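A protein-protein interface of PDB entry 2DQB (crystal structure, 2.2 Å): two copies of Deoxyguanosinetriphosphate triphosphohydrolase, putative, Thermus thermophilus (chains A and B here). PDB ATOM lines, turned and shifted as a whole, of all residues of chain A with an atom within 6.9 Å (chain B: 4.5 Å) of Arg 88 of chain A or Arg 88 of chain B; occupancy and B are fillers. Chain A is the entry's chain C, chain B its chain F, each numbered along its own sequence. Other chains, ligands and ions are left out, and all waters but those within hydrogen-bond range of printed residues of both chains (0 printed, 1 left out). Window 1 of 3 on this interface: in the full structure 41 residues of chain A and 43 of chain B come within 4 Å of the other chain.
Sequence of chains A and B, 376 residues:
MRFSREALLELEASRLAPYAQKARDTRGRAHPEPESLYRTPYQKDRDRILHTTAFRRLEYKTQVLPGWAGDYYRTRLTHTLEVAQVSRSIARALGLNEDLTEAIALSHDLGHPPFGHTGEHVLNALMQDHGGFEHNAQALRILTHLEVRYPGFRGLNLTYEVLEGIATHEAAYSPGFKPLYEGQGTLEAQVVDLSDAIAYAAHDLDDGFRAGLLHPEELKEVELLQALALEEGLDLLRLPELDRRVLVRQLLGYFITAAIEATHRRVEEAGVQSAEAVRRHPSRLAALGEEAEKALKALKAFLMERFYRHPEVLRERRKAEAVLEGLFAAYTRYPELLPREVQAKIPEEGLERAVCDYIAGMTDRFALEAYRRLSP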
ATOM      1  N   GLN A  43      -7.092  31.234 -14.183  1.00  0.00           N
ATOM      2  CA  GLN A  43      -6.362  29.969 -14.156  1.00  0.00           C
ATOM      3  C   GLN A  43      -5.523  30.019 -12.894  1.00  0.00           C
ATOM      4  O   GLN A  43      -5.378  29.029 -12.174  1.00  0.00           O
ATOM      5  CB  GLN A  43      -5.380  29.866 -15.325  1.00  0.00           C
ATOM      6  CG  GLN A  43      -5.928  29.405 -16.655  1.00  0.00           C
ATOM      7  CD  GLN A  43      -4.793  29.127 -17.618  1.00  0.00           C
ATOM      8  OE1 GLN A  43      -4.126  30.045 -18.077  1.00  0.00           O
ATOM      9  NE2 GLN A  43      -4.542  27.851 -17.893  1.00  0.00           N
ATOM     10  N   ARG A  46      -7.432  29.518  -9.803  1.00  0.00           N
ATOM     11  CA  ARG A  46      -7.710  28.092  -9.718  1.00  0.00           C
ATOM     12  C   ARG A  46      -6.504  27.354  -9.101  1.00  0.00           C
ATOM     13  O   ARG A  46      -6.669  26.521  -8.213  1.00  0.00           O
ATOM     14  CB  ARG A  46      -8.034  27.535 -11.105  1.00  0.00           C
ATOM     15  CG  ARG A  46      -8.293  26.039 -11.141  1.00  0.00           C
ATOM     16  CD  ARG A  46      -8.702  25.589 -12.537  1.00  0.00           C
ATOM     17  NE  ARG A  46      -7.699  25.937 -13.539  1.00  0.00           N
ATOM     18  CZ  ARG A  46      -7.925  25.933 -14.848  1.00  0.00           C
ATOM     19  NH1 ARG A  46      -9.113  25.591 -15.315  1.00  0.00           N
ATOM     20  NH2 ARG A  46      -6.982  26.306 -15.691  1.00  0.00           N
ATOM     21  N   GLU A  82     -17.674  17.139  -8.096  1.00  0.00           N
ATOM     22  CA  GLU A  82     -18.897  16.991  -8.854  1.00  0.00           C
ATOM     23  C   GLU A  82     -19.474  18.368  -9.198  1.00  0.00           C
ATOM     24  O   GLU A  82     -19.941  18.592 -10.320  1.00  0.00           O
ATOM     25  CB  GLU A  82     -19.903  16.159  -8.070  1.00  0.00           C
ATOM     26  CG  GLU A  82     -21.222  15.888  -8.797  1.00  0.00           C
ATOM     27  CD  GLU A  82     -21.086  14.981 -10.026  1.00  0.00           C
ATOM     28  OE1 GLU A  82     -20.415  15.374 -11.004  1.00  0.00           O
ATOM     29  OE2 GLU A  82     -21.662  13.875 -10.018  1.00  0.00           O
ATOM     30  N   VAL A  83     -19.437  19.297  -8.244  1.00  0.00           N
ATOM     31  CA  VAL A  83     -19.958  20.642  -8.490  1.00  0.00           C
ATOM     32  C   VAL A  83     -19.120  21.238  -9.626  1.00  0.00           C
ATOM     33  O   VAL A  83     -19.638  21.802 -10.574  1.00  0.00           O
ATOM     34  CB  VAL A  83     -19.836  21.552  -7.222  1.00  0.00           C
ATOM     35  CG1 VAL A  83     -20.329  22.965  -7.523  1.00  0.00           C
ATOM     36  CG2 VAL A  83     -20.669  20.970  -6.090  1.00  0.00           C
ATOM     37  N   ALA A  84     -17.812  21.093  -9.516  1.00  0.00           N
ATOM     38  CA  ALA A  84     -16.907  21.607 -10.517  1.00  0.00           C
ATOM     39  C   ALA A  84     -17.252  21.051 -11.898  1.00  0.00           C
ATOM     40  O   ALA A  84     -17.271  21.787 -12.890  1.00  0.00           O
ATOM     41  CB  ALA A  84     -15.473  21.263 -10.146  1.00  0.00           C
ATOM     42  N   GLN A  85     -17.547  19.754 -11.960  1.00  0.00           N
ATOM     43  CA  GLN A  85     -17.866  19.130 -13.233  1.00  0.00           C
ATOM     44  C   GLN A  85     -19.233  19.498 -13.798  1.00  0.00           C
ATOM     45  O   GLN A  85     -19.360  19.712 -15.000  1.00  0.00           O
ATOM     46  CB  GLN A  85     -17.738  17.615 -13.126  1.00  0.00           C
ATOM     47  CG  GLN A  85     -16.297  17.129 -13.161  1.00  0.00           C
ATOM     48  CD  GLN A  85     -15.776  16.871 -14.573  1.00  0.00           C
ATOM     49  OE1 GLN A  85     -16.467  16.269 -15.407  1.00  0.00           O
ATOM     50  NE2 GLN A  85     -14.536  17.291 -14.836  1.00  0.00           N
ATOM     51  N   VAL A  86     -20.249  19.555 -12.945  1.00  0.00           N
ATOM     52  CA  VAL A  86     -21.591  19.907 -13.385  1.00  0.00           C
ATOM     53  C   VAL A  86     -21.651  21.378 -13.836  1.00  0.00           C
ATOM     54  O   VAL A  86     -22.345  21.714 -14.810  1.00  0.00           O
ATOM     55  CB  VAL A  86     -22.634  19.677 -12.251  1.00  0.00           C
ATOM     56  CG1 VAL A  86     -23.945  20.346 -12.588  1.00  0.00           C
ATOM     57  CG2 VAL A  86     -22.869  18.188 -12.066  1.00  0.00           C
ATOM     58  N   SER A  87     -20.923  22.244 -13.136  1.00  0.00           N
ATOM     59  CA  SER A  87     -20.943  23.649 -13.478  1.00  0.00           C
ATOM     60  C   SER A  87     -20.030  23.983 -14.678  1.00  0.00           C
ATOM     61  O   SER A  87     -20.339  24.893 -15.460  1.00  0.00           O
ATOM     62  CB  SER A  87     -20.592  24.517 -12.249  1.00  0.00           C
ATOM     63  OG  SER A  87     -19.272  24.310 -11.785  1.00  0.00           O
ATOM     64  N   ARG A  88     -18.915  23.266 -14.824  1.00  0.00           N
ATOM     65  CA  ARG A  88     -18.042  23.511 -15.964  1.00  0.00           C
ATOM     66  C   ARG A  88     -18.820  23.137 -17.213  1.00  0.00           C
ATOM     67  O   ARG A  88     -18.721  23.798 -18.249  1.00  0.00           O
ATOM     68  CB  ARG A  88     -16.779  22.655 -15.898  1.00  0.00           C
ATOM     69  CG  ARG A  88     -15.658  23.248 -15.067  1.00  0.00           C
ATOM     70  CD  ARG A  88     -14.528  22.252 -14.947  1.00  0.00           C
ATOM     71  NE  ARG A  88     -13.827  22.034 -16.213  1.00  0.00           N
ATOM     72  CZ  ARG A  88     -12.734  21.278 -16.326  1.00  0.00           C
ATOM     73  NH1 ARG A  88     -12.230  20.665 -15.258  1.00  0.00           N
ATOM     74  NH2 ARG A  88     -12.122  21.157 -17.490  1.00  0.00           N
ATOM     75  N   SER A  89     -19.601  22.075 -17.088  1.00  0.00           N
ATOM     76  CA  SER A  89     -20.418  21.556 -18.174  1.00  0.00           C
ATOM     77  C   SER A  89     -21.571  22.499 -18.584  1.00  0.00           C
ATOM     78  O   SER A  89     -21.852  22.666 -19.772  1.00  0.00           O
ATOM     79  CB  SER A  89     -20.955  20.193 -17.765  1.00  0.00           C
ATOM     80  OG  SER A  89     -21.660  19.577 -18.822  1.00  0.00           O
ATOM     81  N   ILE A  90     -22.234  23.116 -17.608  1.00  0.00           N
ATOM     82  CA  ILE A  90     -23.319  24.042 -17.908  1.00  0.00           C
ATOM     83  C   ILE A  90     -22.685  25.307 -18.472  1.00  0.00           C
ATOM     84  O   ILE A  90     -23.213  25.927 -19.401  1.00  0.00           O
ATOM     85  CB  ILE A  90     -24.144  24.355 -16.643  1.00  0.00           C
ATOM     86  CG1 ILE A  90     -24.858  23.062 -16.207  1.00  0.00           C
ATOM     87  CG2 ILE A  90     -25.195  25.439 -16.925  1.00  0.00           C
ATOM     88  CD1 ILE A  90     -25.545  23.126 -14.853  1.00  0.00           C
ATOM     89  N   ALA A  91     -21.521  25.649 -17.932  1.00  0.00           N
ATOM     90  CA  ALA A  91     -20.808  26.828 -18.357  1.00  0.00           C
ATOM     91  C   ALA A  91     -20.405  26.726 -19.835  1.00  0.00           C
ATOM     92  O   ALA A  91     -20.737  27.600 -20.636  1.00  0.00           O
ATOM     93  CB  ALA A  91     -19.588  27.026 -17.485  1.00  0.00           C
ATOM     94  N   ARG A  92     -19.702  25.657 -20.188  1.00  0.00           N
ATOM     95  CA  ARG A  92     -19.271  25.470 -21.564  1.00  0.00           C
ATOM     96  C   ARG A  92     -20.454  25.550 -22.512  1.00  0.00           C
ATOM     97  O   ARG A  92     -20.381  26.225 -23.537  1.00  0.00           O
ATOM     98  CB  ARG A  92     -18.560  24.125 -21.749  1.00  0.00           C
ATOM     99  CG  ARG A  92     -17.967  23.950 -23.152  1.00  0.00           C
ATOM    100  CD  ARG A  92     -17.049  22.725 -23.269  1.00  0.00           C
ATOM    101  NE  ARG A  92     -15.858  22.818 -22.422  1.00  0.00           N
ATOM    102  CZ  ARG A  92     -14.870  21.925 -22.416  1.00  0.00           C
ATOM    103  NH1 ARG A  92     -14.926  20.872 -23.222  1.00  0.00           N
ATOM    104  NH2 ARG A  92     -13.839  22.070 -21.590  1.00  0.00           N
ATOM    105  N   ALA A  93     -21.554  24.884 -22.171  1.00  0.00           N
ATOM    106  CA  ALA A  93     -22.723  24.909 -23.045  1.00  0.00           C
ATOM    107  C   ALA A  93     -23.284  26.319 -23.248  1.00  0.00           C
ATOM    108  O   ALA A  93     -23.924  26.586 -24.265  1.00  0.00           O
ATOM    109  CB  ALA A  93     -23.818  23.984 -22.500  1.00  0.00           C
ATOM    110  N   LEU A  94     -23.043  27.218 -22.296  1.00  0.00           N
ATOM    111  CA  LEU A  94     -23.562  28.580 -22.412  1.00  0.00           C
ATOM    112  C   LEU A  94     -22.516  29.603 -22.843  1.00  0.00           C
ATOM    113  O   LEU A  94     -22.790  30.798 -22.877  1.00  0.00           O
ATOM    114  CB  LEU A  94     -24.195  29.021 -21.083  1.00  0.00           C
ATOM    115  CG  LEU A  94     -25.385  28.204 -20.566  1.00  0.00           C
ATOM    116  CD1 LEU A  94     -25.750  28.664 -19.167  1.00  0.00           C
ATOM    117  CD2 LEU A  94     -26.572  28.332 -21.494  1.00  0.00           C
ATOM    118  N   LEU A  96     -19.924  30.444 -21.218  1.00  0.00           N
ATOM    119  CA  LEU A  96     -19.440  31.201 -20.080  1.00  0.00           C
ATOM    120  C   LEU A  96     -17.970  30.871 -19.819  1.00  0.00           C
ATOM    121  O   LEU A  96     -17.430  29.910 -20.401  1.00  0.00           O
ATOM    122  CB  LEU A  96     -20.285  30.875 -18.857  1.00  0.00           C
ATOM    123  CG  LEU A  96     -21.779  31.239 -18.941  1.00  0.00           C
ATOM    124  CD1 LEU A  96     -22.518  30.606 -17.764  1.00  0.00           C
ATOM    125  CD2 LEU A  96     -21.949  32.763 -18.962  1.00  0.00           C
ATOM    126  N   GLU A  98     -15.185  29.179 -18.196  1.00  0.00           N
ATOM    127  CA  GLU A  98     -15.033  27.931 -17.473  1.00  0.00           C
ATOM    128  C   GLU A  98     -14.027  28.022 -16.332  1.00  0.00           C
ATOM    129  O   GLU A  98     -14.236  27.419 -15.279  1.00  0.00           O
ATOM    130  CB  GLU A  98     -14.613  26.812 -18.432  1.00  0.00           C
ATOM    131  CG  GLU A  98     -15.323  25.493 -18.172  1.00  0.00           C
ATOM    132  CD  GLU A  98     -14.906  24.401 -19.155  1.00  0.00           C
ATOM    133  OE1 GLU A  98     -15.059  24.621 -20.389  1.00  0.00           O
ATOM    134  OE2 GLU A  98     -14.425  23.334 -18.685  1.00  0.00           O
ATOM    135  N   ASP A  99     -12.931  28.747 -16.532  1.00  0.00           N
ATOM    136  CA  ASP A  99     -11.959  28.871 -15.465  1.00  0.00           C
ATOM    137  C   ASP A  99     -12.575  29.647 -14.300  1.00  0.00           C
ATOM    138  O   ASP A  99     -12.335  29.311 -13.134  1.00  0.00           O
ATOM    139  CB  ASP A  99     -10.695  29.599 -15.914  1.00  0.00           C
ATOM    140  CG  ASP A  99      -9.968  28.886 -17.034  1.00  0.00           C
ATOM    141  OD1 ASP A  99      -9.926  27.627 -17.041  1.00  0.00           O
ATOM    142  OD2 ASP A  99      -9.430  29.603 -17.909  1.00  0.00           O
ATOM    143  N   THR A 101     -15.744  29.791 -13.558  1.00  0.00           N
ATOM    144  CA  THR A 101     -16.713  28.848 -13.001  1.00  0.00           C
ATOM    145  C   THR A 101     -16.019  27.790 -12.122  1.00  0.00           C
ATOM    146  O   THR A 101     -16.414  27.563 -10.980  1.00  0.00           O
ATOM    147  CB  THR A 101     -17.481  28.099 -14.106  1.00  0.00           C
ATOM    148  OG1 THR A 101     -18.119  29.034 -14.979  1.00  0.00           O
ATOM    149  CG2 THR A 101     -18.557  27.199 -13.491  1.00  0.00           C
ATOM    150  N   GLU A 102     -14.986  27.146 -12.663  1.00  0.00           N
ATOM    151  CA  GLU A 102     -14.274  26.129 -11.918  1.00  0.00           C
ATOM    152  C   GLU A 102     -13.655  26.685 -10.645  1.00  0.00           C
ATOM    153  O   GLU A 102     -13.746  26.061  -9.584  1.00  0.00           O
ATOM    154  CB  GLU A 102     -13.190  25.485 -12.795  1.00  0.00           C
ATOM    155  CG  GLU A 102     -12.362  24.421 -12.104  1.00  0.00           C
ATOM    156  CD  GLU A 102     -11.496  23.605 -13.057  1.00  0.00           C
ATOM    157  OE1 GLU A 102     -10.909  24.172 -14.002  1.00  0.00           O
ATOM    158  OE2 GLU A 102     -11.399  22.382 -12.850  1.00  0.00           O
ATOM    159  N   ALA A 103     -13.032  27.856 -10.739  1.00  0.00           N
ATOM    160  CA  ALA A 103     -12.379  28.446  -9.580  1.00  0.00           C
ATOM    161  C   ALA A 103     -13.362  28.702  -8.442  1.00  0.00           C
ATOM    162  O   ALA A 103     -13.034  28.517  -7.267  1.00  0.00           O
ATOM    163  CB  ALA A 103     -11.665  29.730  -9.965  1.00  0.00           C
ATOM    164  N   ALA A 105     -16.357  27.079  -8.080  1.00  0.00           N
ATOM    165  CA  ALA A 105     -16.841  25.783  -7.655  1.00  0.00           C
ATOM    166  C   ALA A 105     -15.838  25.132  -6.700  1.00  0.00           C
ATOM    167  O   ALA A 105     -16.239  24.433  -5.767  1.00  0.00           O
ATOM    168  CB  ALA A 105     -17.077  24.893  -8.860  1.00  0.00           C
ATOM    169  N   LEU A 106     -14.549  25.373  -6.933  1.00  0.00           N
ATOM    170  CA  LEU A 106     -13.487  24.811  -6.103  1.00  0.00           C
ATOM    171  C   LEU A 106     -13.317  25.486  -4.744  1.00  0.00           C
ATOM    172  O   LEU A 106     -12.737  24.899  -3.823  1.00  0.00           O
ATOM    173  CB  LEU A 106     -12.134  24.879  -6.829  1.00  0.00           C
ATOM    174  CG  LEU A 106     -12.014  24.065  -8.133  1.00  0.00           C
ATOM    175  CD1 LEU A 106     -10.634  24.239  -8.743  1.00  0.00           C
ATOM    176  CD2 LEU A 106     -12.249  22.583  -7.830  1.00  0.00           C
ATOM    177  N   VAL A 191     -24.241  29.949 -11.932  1.00  0.00           N
ATOM    178  CA  VAL A 191     -24.281  28.574 -12.424  1.00  0.00           C
ATOM    179  C   VAL A 191     -23.737  27.604 -11.355  1.00  0.00           C
ATOM    180  O   VAL A 191     -24.285  26.509 -11.163  1.00  0.00           O
ATOM    181  CB  VAL A 191     -23.455  28.417 -13.742  1.00  0.00           C
ATOM    182  CG1 VAL A 191     -23.259  26.923 -14.078  1.00  0.00           C
ATOM    183  CG2 VAL A 191     -24.183  29.102 -14.882  1.00  0.00           C
ATOM    184  N   VAL A 192     -22.664  27.999 -10.680  1.00  0.00           N
ATOM    185  CA  VAL A 192     -22.066  27.162  -9.633  1.00  0.00           C
ATOM    186  C   VAL A 192     -23.084  26.826  -8.528  1.00  0.00           C
ATOM    187  O   VAL A 192     -23.221  25.664  -8.120  1.00  0.00           O
ATOM    188  CB  VAL A 192     -20.837  27.860  -9.003  1.00  0.00           C
ATOM    189  CG1 VAL A 192     -20.405  27.131  -7.707  1.00  0.00           C
ATOM    190  CG2 VAL A 192     -19.684  27.893 -10.016  1.00  0.00           C
ATOM    191  N   SER A 195     -25.498  24.355  -9.716  1.00  0.00           N
ATOM    192  CA  SER A 195     -24.869  23.054  -9.887  1.00  0.00           C
ATOM    193  C   SER A 195     -24.673  22.356  -8.533  1.00  0.00           C
ATOM    194  O   SER A 195     -24.709  21.130  -8.436  1.00  0.00           O
ATOM    195  CB  SER A 195     -23.525  23.218 -10.609  1.00  0.00           C
ATOM    196  OG  SER A 195     -23.666  23.981 -11.806  1.00  0.00           O
ATOM    197  N   ARG B  46     -14.014  12.463 -19.785  1.00  0.00           N
ATOM    198  CA  ARG B  46     -13.664  12.992 -18.478  1.00  0.00           C
ATOM    199  C   ARG B  46     -14.799  12.671 -17.499  1.00  0.00           C
ATOM    200  O   ARG B  46     -14.571  12.078 -16.442  1.00  0.00           O
ATOM    201  CB  ARG B  46     -13.424  14.504 -18.562  1.00  0.00           C
ATOM    202  CG  ARG B  46     -13.303  15.222 -17.219  1.00  0.00           C
ATOM    203  CD  ARG B  46     -12.371  16.435 -17.325  1.00  0.00           C
ATOM    204  NE  ARG B  46     -12.666  17.269 -18.496  1.00  0.00           N
ATOM    205  CZ  ARG B  46     -13.752  18.029 -18.623  1.00  0.00           C
ATOM    206  NH1 ARG B  46     -13.943  18.749 -19.728  1.00  0.00           N
ATOM    207  NH2 ARG B  46     -14.637  18.080 -17.633  1.00  0.00           N
ATOM    208  N   ALA B  84      -3.396  16.624 -13.023  1.00  0.00           N
ATOM    209  CA  ALA B  84      -4.406  17.163 -13.909  1.00  0.00           C
ATOM    210  C   ALA B  84      -4.171  18.667 -14.097  1.00  0.00           C
ATOM    211  O   ALA B  84      -4.181  19.157 -15.234  1.00  0.00           O
ATOM    212  CB  ALA B  84      -5.789  16.901 -13.350  1.00  0.00           C
ATOM    213  N   GLN B  85      -3.941  19.375 -12.985  1.00  0.00           N
ATOM    214  CA  GLN B  85      -3.689  20.809 -13.007  1.00  0.00           C
ATOM    215  C   GLN B  85      -2.380  21.152 -13.716  1.00  0.00           C
ATOM    216  O   GLN B  85      -2.312  22.131 -14.480  1.00  0.00           O
ATOM    217  CB  GLN B  85      -3.641  21.376 -11.593  1.00  0.00           C
ATOM    218  CG  GLN B  85      -5.001  21.583 -10.949  1.00  0.00           C
ATOM    219  CD  GLN B  85      -5.813  22.685 -11.620  1.00  0.00           C
ATOM    220  OE1 GLN B  85      -5.325  23.798 -11.817  1.00  0.00           O
ATOM    221  NE2 GLN B  85      -7.060  22.379 -11.957  1.00  0.00           N
ATOM    222  N   VAL B  86      -1.335  20.373 -13.454  1.00  0.00           N
ATOM    223  CA  VAL B  86      -0.051  20.633 -14.101  1.00  0.00           C
ATOM    224  C   VAL B  86      -0.133  20.276 -15.594  1.00  0.00           C
ATOM    225  O   VAL B  86       0.402  20.983 -16.441  1.00  0.00           O
ATOM    226  CB  VAL B  86       1.083  19.848 -13.432  1.00  0.00           C
ATOM    227  CG1 VAL B  86       2.377  19.988 -14.262  1.00  0.00           C
ATOM    228  CG2 VAL B  86       1.293  20.373 -12.015  1.00  0.00           C
ATOM    229  N   SER B  87      -0.818  19.182 -15.891  1.00  0.00           N
ATOM    230  CA  SER B  87      -1.036  18.724 -17.243  1.00  0.00           C
ATOM    231  C   SER B  87      -1.767  19.801 -18.057  1.00  0.00           C
ATOM    232  O   SER B  87      -1.314  20.203 -19.124  1.00  0.00           O
ATOM    233  CB  SER B  87      -1.895  17.465 -17.232  1.00  0.00           C
ATOM    234  OG  SER B  87      -1.119  16.357 -17.612  1.00  0.00           O
ATOM    235  N   ARG B  88      -2.912  20.225 -17.547  1.00  0.00           N
ATOM    236  CA  ARG B  88      -3.717  21.233 -18.199  1.00  0.00           C
ATOM    237  C   ARG B  88      -2.976  22.554 -18.426  1.00  0.00           C
ATOM    238  O   ARG B  88      -3.177  23.188 -19.455  1.00  0.00           O
ATOM    239  CB  ARG B  88      -4.998  21.478 -17.398  1.00  0.00           C
ATOM    240  CG  ARG B  88      -5.951  20.289 -17.358  1.00  0.00           C
ATOM    241  CD  ARG B  88      -7.090  20.519 -16.368  1.00  0.00           C
ATOM    242  NE  ARG B  88      -7.968  21.605 -16.781  1.00  0.00           N
ATOM    243  CZ  ARG B  88      -8.846  22.197 -15.981  1.00  0.00           C
ATOM    244  NH1 ARG B  88      -8.965  21.805 -14.717  1.00  0.00           N
ATOM    245  NH2 ARG B  88      -9.600  23.192 -16.441  1.00  0.00           N
ATOM    246  N   SER B  89      -2.119  22.959 -17.493  1.00  0.00           N
ATOM    247  CA  SER B  89      -1.380  24.212 -17.642  1.00  0.00           C
ATOM    248  C   SER B  89      -0.381  24.136 -18.795  1.00  0.00           C
ATOM    249  O   SER B  89      -0.276  25.063 -19.616  1.00  0.00           O
ATOM    250  CB  SER B  89      -0.645  24.569 -16.344  1.00  0.00           C
ATOM    251  OG  SER B  89      -1.429  25.455 -15.561  1.00  0.00           O
ATOM    252  N   ILE B  90       0.349  23.027 -18.853  1.00  0.00           N
ATOM    253  CA  ILE B  90       1.322  22.820 -19.907  1.00  0.00           C
ATOM    254  C   ILE B  90       0.555  22.805 -21.224  1.00  0.00           C
ATOM    255  O   ILE B  90       0.859  23.563 -22.136  1.00  0.00           O
ATOM    256  CB  ILE B  90       2.054  21.462 -19.752  1.00  0.00           C
ATOM    257  CG1 ILE B  90       2.655  21.316 -18.342  1.00  0.00           C
ATOM    258  CG2 ILE B  90       3.170  21.360 -20.789  1.00  0.00           C
ATOM    259  CD1 ILE B  90       3.847  22.174 -18.080  1.00  0.00           C
ATOM    260  N   ALA B  91      -0.446  21.936 -21.304  1.00  0.00           N
ATOM    261  CA  ALA B  91      -1.258  21.782 -22.494  1.00  0.00           C
ATOM    262  C   ALA B  91      -1.736  23.129 -23.065  1.00  0.00           C
ATOM    263  O   ALA B  91      -1.311  23.538 -24.140  1.00  0.00           O
ATOM    264  CB  ALA B  91      -2.459  20.884 -22.193  1.00  0.00           C
ATOM    265  N   ARG B  92      -2.617  23.808 -22.335  1.00  0.00           N
ATOM    266  CA  ARG B  92      -3.150  25.095 -22.771  1.00  0.00           C
ATOM    267  C   ARG B  92      -2.058  25.991 -23.327  1.00  0.00           C
ATOM    268  O   ARG B  92      -2.190  26.552 -24.420  1.00  0.00           O
ATOM    269  CB  ARG B  92      -3.843  25.813 -21.617  1.00  0.00           C
ATOM    270  CG  ARG B  92      -4.473  27.123 -22.054  1.00  0.00           C
ATOM    271  CD  ARG B  92      -5.159  27.842 -20.898  1.00  0.00           C
ATOM    272  NE  ARG B  92      -6.318  27.088 -20.430  1.00  0.00           N
ATOM    273  CZ  ARG B  92      -7.284  27.604 -19.681  1.00  0.00           C
ATOM    274  NH1 ARG B  92      -7.236  28.880 -19.312  1.00  0.00           N
ATOM    275  NH2 ARG B  92      -8.295  26.837 -19.298  1.00  0.00           N
ATOM    276  N   GLU B  98      -6.951  20.280 -24.049  1.00  0.00           N
ATOM    277  CA  GLU B  98      -6.959  20.251 -22.597  1.00  0.00           C
ATOM    278  C   GLU B  98      -7.881  19.141 -22.066  1.00  0.00           C
ATOM    279  O   GLU B  98      -7.584  18.539 -21.034  1.00  0.00           O
ATOM    280  CB  GLU B  98      -7.410  21.614 -22.053  1.00  0.00           C
ATOM    281  CG  GLU B  98      -6.661  22.082 -20.833  1.00  0.00           C
ATOM    282  CD  GLU B  98      -7.146  23.442 -20.339  1.00  0.00           C
ATOM    283  OE1 GLU B  98      -7.323  24.346 -21.188  1.00  0.00           O
ATOM    284  OE2 GLU B  98      -7.338  23.608 -19.110  1.00  0.00           O
ATOM    285  N   THR B 101      -6.075  15.879 -22.408  1.00  0.00           N
ATOM    286  CA  THR B 101      -5.027  15.905 -21.405  1.00  0.00           C
ATOM    287  C   THR B 101      -5.621  15.568 -20.030  1.00  0.00           C
ATOM    288  O   THR B 101      -5.140  14.645 -19.341  1.00  0.00           O
ATOM    289  CB  THR B 101      -4.357  17.284 -21.377  1.00  0.00           C
ATOM    290  OG1 THR B 101      -3.813  17.562 -22.676  1.00  0.00           O
ATOM    291  CG2 THR B 101      -3.233  17.333 -20.362  1.00  0.00           C
ATOM    292  N   GLU B 102      -6.681  16.294 -19.660  1.00  0.00           N
ATOM    293  CA  GLU B 102      -7.358  16.093 -18.388  1.00  0.00           C
ATOM    294  C   GLU B 102      -7.835  14.658 -18.256  1.00  0.00           C
ATOM    295  O   GLU B 102      -7.512  13.996 -17.266  1.00  0.00           O
ATOM    296  CB  GLU B 102      -8.563  17.041 -18.232  1.00  0.00           C
ATOM    297  CG  GLU B 102      -8.844  17.411 -16.776  1.00  0.00           C
ATOM    298  CD  GLU B 102     -10.025  18.371 -16.579  1.00  0.00           C
ATOM    299  OE1 GLU B 102     -10.346  19.178 -17.488  1.00  0.00           O
ATOM    300  OE2 GLU B 102     -10.621  18.326 -15.482  1.00  0.00           O
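The guanidinium group of Arg 92 of chain B lies close to the side-chain amide nitrogen of Gln 43 of chain A, 3.2 Å away.
The guanidinium group (NH2) of Arg 88 of chain B sits close to the guanidinium group (NH1) of Arg 46 of chain A (2.7 Å).
The side-chain amide nitrogen of Gln 85 of chain A lies close to the guanidinium group of Arg 46 of chain B (2.9 Å).
The guanidinium group of Arg 88 of chain A is in salt-bridge range of the side-chain carboxylate of Glu 102 of chain B.
OD2 of Asp 99 of chain A lies within salt-bridge range of NH1 of Arg 92 of chain B (2.7 Å).
OE1 of Glu 102 of chain A is in salt-bridge range of NH2 of Arg 88 of chain B (2.9 Å).
The guanidinium group (NH2) of Arg 88 of chain B sits close to the guanidinium group (NH2) of Arg 88 of chain A (3.4 Å).
The guanidinium group of Arg 88 of chain A lies within salt-bridge range of the side-chain carboxylate of Glu 98 of chain A.
The guanidinium group (NH1) of Arg 88 of chain A is in salt-bridge range of the side-chain carboxylate (OE2) of Glu 102 of chain A (3.1 Å).
The guanidinium group of Arg 92 of chain A is in salt-bridge range of the side-chain carboxylate of Glu 98 of chain A, 2.8 Å away.
OE1 of Glu 102 of chain B is in salt-bridge range of NE of Arg 46 of chain B.
The side-chain carboxylate (OE2) of Glu 98 of chain B lies within salt-bridge range of the guanidinium group (NE) of Arg 88 of chain B (3.1 Å).
The guanidinium group of Arg 88 of chain B lies within salt-bridge range of the side-chain carboxylate of Glu 102 of chain B, 3.5 Å away.
Among the printed residues, pairs that only touch across the chains: Arg 46 of chain A with Gln 85 of chain B (3.6 Å), Arg 88 of chain A with Arg 46 of chain B (3.7 Å), Arg 92 of chain A with Arg 46 of chain B (3.8 Å) and Arg 46 of chain A with Arg 92 of chain B (3.9 Å).
Of the printed residues of chain B, Gln 43 of chain A touches Arg 92.
Of the printed residues of chain B, Arg 46 of chain A touches Gln 85, Arg 88 and Arg 92.
Arg 88 of chain A touches just these residues of chain B: Arg 46 (3.7 Å), Arg 88 (3.4 Å) and Glu 102 (2.7 Å).
Printed residues of chain B within 4 Å of Arg 92 of chain A: Arg 46.
Ser 195 of chain A touches none of the printed residues of chain B.
Arg 88 of chain B touches just these residues of chain A: Arg 46 (2.7 Å), Arg 88 (3.4 Å) and Glu 102 (2.9 Å).
Of the printed residues of chain A, Glu 102 of chain B touches Arg 88.
Among the printed residues, 11 pairs touch across the chains.
Arg 46 of chain A touches Gln 85 of chain B, and with the chains exchanged Gln 85 of chain A touches Arg 46 of chain B.
Arg 46 of chain A touches Arg 92 of chain B, and with the chains exchanged Arg 92 of chain A touches Arg 46 of chain B.
Arg 88 of chain B touches its own counterpart, Arg 88 of chain A.
Arg 88 of chain A touches Glu 102 of chain B, and with the chains exchanged Glu 102 of chain A touches Arg 88 of chain B.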
